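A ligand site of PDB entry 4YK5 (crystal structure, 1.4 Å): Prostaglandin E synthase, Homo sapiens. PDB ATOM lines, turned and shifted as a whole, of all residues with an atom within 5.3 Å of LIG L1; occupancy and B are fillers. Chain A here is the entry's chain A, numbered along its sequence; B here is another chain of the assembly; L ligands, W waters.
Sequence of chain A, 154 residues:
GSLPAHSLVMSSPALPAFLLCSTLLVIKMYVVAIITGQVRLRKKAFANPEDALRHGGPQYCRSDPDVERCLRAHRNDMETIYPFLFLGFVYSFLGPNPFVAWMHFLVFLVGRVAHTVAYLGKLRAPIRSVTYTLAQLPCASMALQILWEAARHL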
ATOM      1  N   ARG A  72      25.509 -15.261 -26.840  1.00  0.00           N
ATOM      2  CA  ARG A  72      24.206 -15.933 -26.825  1.00  0.00           C
ATOM      3  C   ARG A  72      23.094 -15.044 -27.372  1.00  0.00           C
ATOM      4  O   ARG A  72      22.244 -15.506 -28.140  1.00  0.00           O
ATOM      5  CB  ARG A  72      23.828 -16.440 -25.434  1.00  0.00           C
ATOM      6  CG  ARG A  72      24.652 -17.616 -24.955  1.00  0.00           C
ATOM      7  CD  ARG A  72      24.018 -18.330 -23.768  1.00  0.00           C
ATOM      8  NE  ARG A  72      23.954 -17.511 -22.553  1.00  0.00           N
ATOM      9  CZ  ARG A  72      24.967 -17.327 -21.706  1.00  0.00           C
ATOM     10  NH1 ARG A  72      26.149 -17.898 -21.932  1.00  0.00           N
ATOM     11  NH2 ARG A  72      24.797 -16.571 -20.633  1.00  0.00           N
ATOM     12  N   ALA A  73      23.097 -13.768 -26.975  1.00  0.00           N
ATOM     13  CA  ALA A  73      22.110 -12.822 -27.473  1.00  0.00           C
ATOM     14  C   ALA A  73      22.242 -12.679 -28.998  1.00  0.00           C
ATOM     15  O   ALA A  73      21.251 -12.715 -29.721  1.00  0.00           O
ATOM     16  CB  ALA A  73      22.258 -11.466 -26.795  1.00  0.00           C
ATOM     17  N   ARG A  75      23.632 -14.851 -31.066  1.00  0.00           N
ATOM     18  CA  ARG A  75      23.233 -16.102 -31.695  1.00  0.00           C
ATOM     19  C   ARG A  75      21.709 -16.237 -31.748  1.00  0.00           C
ATOM     20  O   ARG A  75      21.145 -16.623 -32.772  1.00  0.00           O
ATOM     21  CB  ARG A  75      23.871 -17.297 -30.997  1.00  0.00           C
ATOM     22  CG  ARG A  75      23.560 -18.592 -31.718  1.00  0.00           C
ATOM     23  CD  ARG A  75      24.133 -19.805 -31.024  1.00  0.00           C
ATOM     24  NE  ARG A  75      23.464 -20.980 -31.565  1.00  0.00           N
ATOM     25  CZ  ARG A  75      24.034 -22.165 -31.752  1.00  0.00           C
ATOM     26  NH1 ARG A  75      23.303 -23.138 -32.268  1.00  0.00           N
ATOM     27  NH2 ARG A  75      25.321 -22.376 -31.466  1.00  0.00           N
ATOM     28  N   ASN A  76      21.031 -15.900 -30.647  1.00  0.00           N
ATOM     29  CA  ASN A  76      19.586 -15.951 -30.647  1.00  0.00           C
ATOM     30  C   ASN A  76      18.981 -15.025 -31.708  1.00  0.00           C
ATOM     31  O   ASN A  76      18.033 -15.400 -32.393  1.00  0.00           O
ATOM     32  CB  ASN A  76      19.009 -15.688 -29.247  1.00  0.00           C
ATOM     33  CG  ASN A  76      17.540 -16.042 -29.160  1.00  0.00           C
ATOM     34  OD1 ASN A  76      16.684 -15.222 -29.496  1.00  0.00           O
ATOM     35  ND2 ASN A  76      17.240 -17.260 -28.719  1.00  0.00           N
ATOM     36  N   GLU A  79      19.166 -16.766 -34.930  1.00  0.00           N
ATOM     37  CA  GLU A  79      18.158 -17.831 -34.969  1.00  0.00           C
ATOM     38  C   GLU A  79      16.740 -17.321 -35.254  1.00  0.00           C
ATOM     39  O   GLU A  79      15.858 -18.101 -35.625  1.00  0.00           O
ATOM     40  CB  GLU A  79      18.162 -18.633 -33.654  1.00  0.00           C
ATOM     41  CG  GLU A  79      19.453 -19.393 -33.409  1.00  0.00           C
ATOM     42  CD  GLU A  79      19.562 -20.004 -32.018  1.00  0.00           C
ATOM     43  OE1 GLU A  79      18.630 -19.875 -31.203  1.00  0.00           O
ATOM     44  OE2 GLU A  79      20.613 -20.623 -31.724  1.00  0.00           O
ATOM     45  N   HIS A 115      13.833  -8.435 -26.063  1.00  0.00           N
ATOM     46  CA  HIS A 115      14.639  -9.649 -25.850  1.00  0.00           C
ATOM     47  C   HIS A 115      16.095  -9.312 -25.561  1.00  0.00           C
ATOM     48  O   HIS A 115      16.675  -9.831 -24.606  1.00  0.00           O
ATOM     49  CB  HIS A 115      14.547 -10.596 -27.051  1.00  0.00           C
ATOM     50  CG  HIS A 115      15.230 -11.903 -26.841  1.00  0.00           C
ATOM     51  ND1 HIS A 115      16.581 -12.090 -27.106  1.00  0.00           N
ATOM     52  CD2 HIS A 115      14.769 -13.096 -26.399  1.00  0.00           C
ATOM     53  CE1 HIS A 115      16.903 -13.343 -26.825  1.00  0.00           C
ATOM     54  NE2 HIS A 115      15.822 -13.972 -26.403  1.00  0.00           N
ATOM     55  N   TYR A 119      18.030  -9.948 -22.147  1.00  0.00           N
ATOM     56  CA  TYR A 119      19.187 -10.839 -22.151  1.00  0.00           C
ATOM     57  C   TYR A 119      20.419 -10.153 -21.578  1.00  0.00           C
ATOM     58  O   TYR A 119      21.019 -10.627 -20.614  1.00  0.00           O
ATOM     59  CB  TYR A 119      19.510 -11.361 -23.561  1.00  0.00           C
ATOM     60  CG  TYR A 119      19.959 -12.815 -23.580  1.00  0.00           C
ATOM     61  CD1 TYR A 119      20.473 -13.415 -22.440  1.00  0.00           C
ATOM     62  CD2 TYR A 119      19.857 -13.587 -24.740  1.00  0.00           C
ATOM     63  CE1 TYR A 119      20.864 -14.737 -22.433  1.00  0.00           C
ATOM     64  CE2 TYR A 119      20.264 -14.916 -24.748  1.00  0.00           C
ATOM     65  CZ  TYR A 119      20.762 -15.489 -23.583  1.00  0.00           C
ATOM     66  OH  TYR A 119      21.154 -16.814 -23.539  1.00  0.00           O
ATOM     67  N   ARG A 128      12.776 -12.720 -20.543  1.00  0.00           N
ATOM     68  CA  ARG A 128      13.409 -12.969 -21.842  1.00  0.00           C
ATOM     69  C   ARG A 128      12.631 -14.016 -22.649  1.00  0.00           C
ATOM     70  O   ARG A 128      12.352 -13.810 -23.830  1.00  0.00           O
ATOM     71  CB  ARG A 128      14.863 -13.401 -21.673  1.00  0.00           C
ATOM     72  CG  ARG A 128      15.623 -13.499 -22.982  1.00  0.00           C
ATOM     73  CD  ARG A 128      16.895 -14.317 -22.831  1.00  0.00           C
ATOM     74  NE  ARG A 128      16.629 -15.741 -22.710  1.00  0.00           N
ATOM     75  CZ  ARG A 128      16.720 -16.456 -21.591  1.00  0.00           C
ATOM     76  NH1 ARG A 128      17.081 -15.887 -20.445  1.00  0.00           N
ATOM     77  NH2 ARG A 128      16.440 -17.747 -21.617  1.00  0.00           N
ATOM     78  N   SER A 129      12.277 -15.127 -22.002  1.00  0.00           N
ATOM     79  CA  SER A 129      11.539 -16.195 -22.678  1.00  0.00           C
ATOM     80  C   SER A 129      10.203 -15.707 -23.249  1.00  0.00           C
ATOM     81  O   SER A 129       9.819 -16.085 -24.351  1.00  0.00           O
ATOM     82  CB  SER A 129      11.326 -17.385 -21.749  1.00  0.00           C
ATOM     83  OG  SER A 129      12.581 -17.909 -21.336  1.00  0.00           O
ATOM     84  N   TYR A 132      10.836 -13.512 -26.403  1.00  0.00           N
ATOM     85  CA  TYR A 132      11.121 -14.427 -27.515  1.00  0.00           C
ATOM     86  C   TYR A 132       9.833 -15.011 -28.091  1.00  0.00           C
ATOM     87  O   TYR A 132       9.640 -15.026 -29.308  1.00  0.00           O
ATOM     88  CB  TYR A 132      12.057 -15.546 -27.030  1.00  0.00           C
ATOM     89  CG  TYR A 132      12.077 -16.805 -27.863  1.00  0.00           C
ATOM     90  CD1 TYR A 132      12.796 -16.867 -29.074  1.00  0.00           C
ATOM     91  CD2 TYR A 132      11.401 -17.951 -27.448  1.00  0.00           C
ATOM     92  CE1 TYR A 132      12.825 -18.041 -29.819  1.00  0.00           C
ATOM     93  CE2 TYR A 132      11.426 -19.117 -28.186  1.00  0.00           C
ATOM     94  CZ  TYR A 132      12.138 -19.162 -29.371  1.00  0.00           C
ATOM     95  OH  TYR A 132      12.149 -20.337 -30.092  1.00  0.00           O
ATOM     96  N   ALA B  33      14.563 -25.278 -32.577  1.00  0.00           N
ATOM     97  CA  ALA B  33      14.566 -24.343 -31.453  1.00  0.00           C
ATOM     98  C   ALA B  33      13.649 -24.819 -30.325  1.00  0.00           C
ATOM     99  O   ALA B  33      14.029 -24.756 -29.143  1.00  0.00           O
ATOM    100  CB  ALA B  33      14.164 -22.952 -31.912  1.00  0.00           C
ATOM    101  N   ILE B  34      12.452 -25.294 -30.686  1.00  0.00           N
ATOM    102  CA  ILE B  34      11.476 -25.778 -29.704  1.00  0.00           C
ATOM    103  C   ILE B  34      12.012 -27.018 -28.986  1.00  0.00           C
ATOM    104  O   ILE B  34      11.953 -27.109 -27.757  1.00  0.00           O
ATOM    105  CB  ILE B  34      10.105 -26.037 -30.362  1.00  0.00           C
ATOM    106  CG1 ILE B  34       9.491 -24.714 -30.844  1.00  0.00           C
ATOM    107  CG2 ILE B  34       9.154 -26.743 -29.403  1.00  0.00           C
ATOM    108  CD1 ILE B  34       8.399 -24.864 -31.880  1.00  0.00           C
ATOM    109  N   THR B  36      15.138 -27.824 -28.595  1.00  0.00           N
ATOM    110  CA  THR B  36      16.240 -27.369 -27.739  1.00  0.00           C
ATOM    111  C   THR B  36      15.717 -26.910 -26.383  1.00  0.00           C
ATOM    112  O   THR B  36      16.255 -27.312 -25.342  1.00  0.00           O
ATOM    113  CB  THR B  36      17.042 -26.223 -28.406  1.00  0.00           C
ATOM    114  OG1 THR B  36      17.512 -26.642 -29.694  1.00  0.00           O
ATOM    115  CG2 THR B  36      18.250 -25.838 -27.551  1.00  0.00           C
ATOM    116  N   GLY B  37      14.674 -26.082 -26.382  1.00  0.00           N
ATOM    117  CA  GLY B  37      14.075 -25.585 -25.152  1.00  0.00           C
ATOM    118  C   GLY B  37      13.539 -26.701 -24.282  1.00  0.00           C
ATOM    119  O   GLY B  37      13.721 -26.686 -23.057  1.00  0.00           O
ATOM    120  N   ARG B  40      16.425 -28.546 -22.674  1.00  0.00           N
ATOM    121  CA  ARG B  40      16.915 -27.737 -21.559  1.00  0.00           C
ATOM    122  C   ARG B  40      16.080 -27.939 -20.298  1.00  0.00           C
ATOM    123  O   ARG B  40      16.636 -28.115 -19.208  1.00  0.00           O
ATOM    124  CB  ARG B  40      16.934 -26.248 -21.912  1.00  0.00           C
ATOM    125  CG  ARG B  40      18.003 -25.839 -22.915  1.00  0.00           C
ATOM    126  CD  ARG B  40      18.122 -24.323 -22.971  1.00  0.00           C
ATOM    127  NE  ARG B  40      19.178 -23.843 -23.865  1.00  0.00           N
ATOM    128  CZ  ARG B  40      20.479 -23.838 -23.572  1.00  0.00           C
ATOM    129  NH1 ARG B  40      20.909 -24.292 -22.407  1.00  0.00           N
ATOM    130  NH2 ARG B  40      21.348 -23.363 -24.448  1.00  0.00           N
ATOM    131  N   ALA B  47      21.407 -22.074 -19.883  1.00  0.00           N
ATOM    132  CA  ALA B  47      22.578 -21.286 -20.233  1.00  0.00           C
ATOM    133  C   ALA B  47      22.786 -20.100 -19.302  1.00  0.00           C
ATOM    134  O   ALA B  47      23.884 -19.541 -19.249  1.00  0.00           O
ATOM    135  CB  ALA B  47      22.484 -20.826 -21.671  1.00  0.00           C
ATOM    136  N   ASN B  48      21.740 -19.710 -18.581  1.00  0.00           N
ATOM    137  CA  ASN B  48      21.724 -18.468 -17.824  1.00  0.00           C
ATOM    138  C   ASN B  48      21.334 -18.689 -16.374  1.00  0.00           C
ATOM    139  O   ASN B  48      20.400 -19.440 -16.099  1.00  0.00           O
ATOM    140  CB  ASN B  48      20.735 -17.498 -18.452  1.00  0.00           C
ATOM    141  CG  ASN B  48      21.012 -17.273 -19.929  1.00  0.00           C
ATOM    142  OD1 ASN B  48      22.060 -16.745 -20.287  1.00  0.00           O
ATOM    143  ND2 ASN B  48      20.085 -17.682 -20.776  1.00  0.00           N
ATOM    144  N   LEU B  71      21.994 -27.529 -30.286  1.00  0.00           N
ATOM    145  CA  LEU B  71      22.608 -26.284 -30.740  1.00  0.00           C
ATOM    146  C   LEU B  71      23.470 -26.472 -31.979  1.00  0.00           C
ATOM    147  O   LEU B  71      23.484 -25.623 -32.854  1.00  0.00           O
ATOM    148  CB  LEU B  71      23.406 -25.614 -29.613  1.00  0.00           C
ATOM    149  CG  LEU B  71      22.584 -24.984 -28.480  1.00  0.00           C
ATOM    150  CD1 LEU B  71      23.484 -24.702 -27.288  1.00  0.00           C
ATOM    151  CD2 LEU B  71      21.891 -23.706 -28.945  1.00  0.00           C
ATOM    152  N   HIS B  74      21.094 -26.791 -34.949  1.00  0.00           N
ATOM    153  CA  HIS B  74      20.579 -25.472 -35.264  1.00  0.00           C
ATOM    154  C   HIS B  74      21.638 -24.605 -35.942  1.00  0.00           C
ATOM    155  O   HIS B  74      21.354 -23.907 -36.915  1.00  0.00           O
ATOM    156  CB  HIS B  74      20.064 -24.788 -33.997  1.00  0.00           C
ATOM    157  CG  HIS B  74      19.033 -23.729 -34.241  1.00  0.00           C
ATOM    158  ND1 HIS B  74      18.241 -23.232 -33.232  1.00  0.00           N
ATOM    159  CD2 HIS B  74      18.649 -23.093 -35.372  1.00  0.00           C
ATOM    160  CE1 HIS B  74      17.417 -22.326 -33.729  1.00  0.00           C
ATOM    161  NE2 HIS B  74      17.645 -22.226 -35.027  1.00  0.00           N
HETATM  162  N1  LIG L   1      18.957 -21.766 -29.134  1.00  0.00           N
HETATM  163  C1  LIG L   1      17.839 -21.502 -28.181  1.00  0.00           C
HETATM  164  C2  LIG L   1      18.203 -21.957 -26.790  1.00  0.00           C
HETATM  165  O1  LIG L   1      17.476 -21.626 -25.830  1.00  0.00           O
HETATM  166  O2  LIG L   1      19.249 -22.639 -26.642  1.00  0.00           O
HETATM  167  C3  LIG L   1      16.556 -22.156 -28.704  1.00  0.00           C
HETATM  168  C4  LIG L   1      15.263 -21.749 -27.978  1.00  0.00           C
HETATM  169  C5  LIG L   1      15.181 -20.251 -27.727  1.00  0.00           C
HETATM  170  O3  LIG L   1      15.410 -19.450 -28.626  1.00  0.00           O
HETATM  171  N2  LIG L   1      14.852 -19.881 -26.492  1.00  0.00           N
HETATM  172  C6  LIG L   1      14.726 -18.487 -26.081  1.00  0.00           C
HETATM  173  C7  LIG L   1      16.040 -17.861 -25.670  1.00  0.00           C
HETATM  174  O4  LIG L   1      16.071 -16.664 -25.396  1.00  0.00           O
HETATM  175  C8  LIG L   1      13.725 -18.357 -24.947  1.00  0.00           C
HETATM  176  S1  LIG L   1      14.185 -19.323 -23.483  1.00  0.00           S
HETATM  177  N3  LIG L   1      17.107 -18.651 -25.616  1.00  0.00           N
HETATM  178  C9  LIG L   1      18.391 -18.177 -25.131  1.00  0.00           C
HETATM  179  C10 LIG L   1      19.530 -18.407 -26.095  1.00  0.00           C
HETATM  180  O5  LIG L   1      19.286 -18.772 -27.270  1.00  0.00           O
HETATM  181  O6  LIG L   1      20.704 -18.227 -25.670  1.00  0.00           O
HETATM  182  O1  LG2 L   2       6.708 -19.427 -16.358  1.00  0.00           O
HETATM  183  C1  LG2 L   2       8.488 -22.964 -24.888  1.00  0.00           C
HETATM  184  O2  LG2 L   2       8.865 -19.802 -16.785  1.00  0.00           O
HETATM  185  C2  LG2 L   2       8.101 -21.721 -25.431  1.00  0.00           C
HETATM  186  C3  LG2 L   2       8.455 -20.575 -20.912  1.00  0.00           C
HETATM  187  N1  LG2 L   2       8.724 -21.890 -21.288  1.00  0.00           N
HETATM  188  C4  LG2 L   2       7.976 -20.624 -24.543  1.00  0.00           C
HETATM  189  C5  LG2 L   2       8.201 -20.770 -23.153  1.00  0.00           C
HETATM  190  C6  LG2 L   2       7.778 -18.410 -22.194  1.00  0.00           C
HETATM  191  C7  LG2 L   2       8.136 -19.860 -22.060  1.00  0.00           C
HETATM  192 CL1  LG2 L   2      15.463 -22.299 -21.209  1.00  0.00          CL
HETATM  193  C8  LG2 L   2      13.765 -22.457 -21.014  1.00  0.00           C
HETATM  194  C9  LG2 L   2      13.059 -23.313 -21.866  1.00  0.00           C
HETATM  195  C10 LG2 L   2      11.676 -23.437 -21.708  1.00  0.00           C
HETATM  196  C11 LG2 L   2      13.122 -21.735 -20.007  1.00  0.00           C
HETATM  197  C12 LG2 L   2      11.735 -21.872 -19.853  1.00  0.00           C
HETATM  198  C13 LG2 L   2      11.001 -22.722 -20.696  1.00  0.00           C
HETATM  199  C14 LG2 L   2       9.507 -22.860 -20.510  1.00  0.00           C
HETATM  200  C15 LG2 L   2       8.565 -22.021 -22.664  1.00  0.00           C
HETATM  201  C16 LG2 L   2       8.542 -20.070 -19.484  1.00  0.00           C
HETATM  202  C17 LG2 L   2       7.274 -20.217 -18.596  1.00  0.00           C
HETATM  203  C18 LG2 L   2       7.571 -19.778 -17.159  1.00  0.00           C
HETATM  204  C19 LG2 L   2       6.633 -21.621 -18.605  1.00  0.00           C
HETATM  205  C20 LG2 L   2       6.190 -19.250 -19.149  1.00  0.00           C
HETATM  206  C21 LG2 L   2       8.716 -23.137 -23.513  1.00  0.00           C
HETATM  207  C22 LG2 L   2       7.890 -21.546 -26.880  1.00  0.00           C
HETATM  208  C23 LG2 L   2       7.462 -22.586 -27.722  1.00  0.00           C
HETATM  209  C24 LG2 L   2       7.280 -22.377 -29.109  1.00  0.00           C
HETATM  210  C25 LG2 L   2       7.537 -21.111 -29.666  1.00  0.00           C
HETATM  211  C26 LG2 L   2       7.974 -20.082 -28.822  1.00  0.00           C
HETATM  212  F1  LG2 L   2       8.231 -18.860 -29.311  1.00  0.00           F
HETATM  213  C27 LG2 L   2       8.145 -20.284 -27.450  1.00  0.00           C
HETATM  214  C28 LG2 L   2       7.379 -20.834 -31.100  1.00  0.00           C
HETATM  215  C29 LG2 L   2       6.169 -20.367 -31.700  1.00  0.00           C
HETATM  216  C30 LG2 L   2       4.906 -20.109 -30.913  1.00  0.00           C
HETATM  217  C31 LG2 L   2       6.138 -20.134 -33.084  1.00  0.00           C
HETATM  218  C32 LG2 L   2       7.265 -20.339 -33.885  1.00  0.00           C
HETATM  219  C33 LG2 L   2       8.455 -20.791 -33.316  1.00  0.00           C
HETATM  220  C34 LG2 L   2       8.502 -21.029 -31.932  1.00  0.00           C
HETATM  221  O   HOH W   1      22.049 -20.869 -25.316  1.00  0.00           O
HETATM  222  O   HOH W   2      18.688 -24.122 -30.605  1.00  0.00           O
HETATM  223  O   HOH W   3      21.426 -19.333 -29.052  1.00  0.00           O
HETATM  224  O   HOH W   4      11.280 -20.585 -24.306  1.00  0.00           O
HETATM  225  O   HOH W   5      19.812 -20.764 -23.630  1.00  0.00           O
HETATM  226  O   HOH W   6      17.285 -20.862 -23.205  1.00  0.00           O
HETATM  227  O   HOH W   7      15.870 -19.684 -31.362  1.00  0.00           O
HETATM  228  O   HOH W   8      14.712 -22.366 -24.694  1.00  0.00           O
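The guanidinium group (NE) of Arg 40 of chain B lies within salt-bridge range of an oxygen (O2) of LIG L1, 3.0 Å away. The side-chain hydroxyl (OG) of Ser 129 lies close to a sulfur (S1) of LIG L1, 3.0 Å away. O6 of LIG L1 is in hydrogen-bond range of OH of Tyr 119 (2.6 Å). A ring nitrogen (NE2) of His 115 is in hydrogen-bond range of an oxygen (O4) of LIG L1, at 2.9 Å. The side-chain amide nitrogen of Asn 76 lies within hydrogen-bond range of an oxygen (O3) of LIG L1 (2.9 Å). NE of Arg 128 sits at hydrogen-bond distance from O4 of LIG L1, 2.9 Å away. The side-chain carboxylate of Glu 79 lies within salt-bridge range of a nitrogen (N1) of LIG L1.
The side-chain carboxylate of Glu 79 is in salt-bridge range of the guanidinium group of Arg 75 (2.9 Å). The side-chain hydroxyl of Tyr 119 is in hydrogen-bond range of the side-chain amide nitrogen of Asn 48 of chain B (3.1 Å). The side-chain amide oxygen of Asn 76 sits close to a ring nitrogen (NE2) of His 115 (3.4 Å). O of Ala 47 of chain B is in hydrogen-bond range of NH2 of Arg 72, 3.4 Å away. The guanidinium group (NH2) of Arg 72 is in hydrogen-bond range of the side-chain amide oxygen (OD1) of Asn 48 of chain B. The guanidinium group (NE) of Arg 72 sits at hydrogen-bond distance from the side-chain hydroxyl (OH) of Tyr 119 (3.0 Å). The backbone carbonyl oxygen (O) of Leu 71 of chain B lies within hydrogen-bond range of the guanidinium group (NH1) of Arg 75, at 2.6 Å.
Arg 72 touches LIG L1 (CB to O6, 3.6 Å). Tyr 132 touches LIG L1 (CE1 to O3, 3.2 Å). Ala 33 of chain B touches LIG L1 (O to C4, 3.5 Å). CG2 of Thr 36 of chain B touches O2 of LIG L1 (3.5 Å). Leu 71 of chain B touches LIG L1 (CD2 to N1, 3.5 Å). Hydrophobic or aromatic side chains that line LIG L1: His 115, Tyr 119, Tyr 132 and Leu 71 of chain B.
Water W7 bridges the side-chain carboxylate of Glu 79 (2.8 Å) and an oxygen (O3) of LIG L1 (2.8 Å). Water W2 lies within hydrogen-bond range of a nitrogen (N1) of LIG L1, a ring nitrogen (ND1) of His 74 of chain B and the side-chain hydroxyl (OG1) of Thr 36 of chain B. Water W3 bridges O5 of LIG L1 (2.8 Å) and OE2 of Glu 79 (3.1 Å). Water W1 lies within hydrogen-bond range of NH2 of Arg 40 of chain B and O6 of LIG L1. Water W5 lies within hydrogen-bond range of the guanidinium group (NH2) of Arg 40 of chain B (3.1 Å) and an oxygen (O1) of LIG L1 (3.3 Å).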
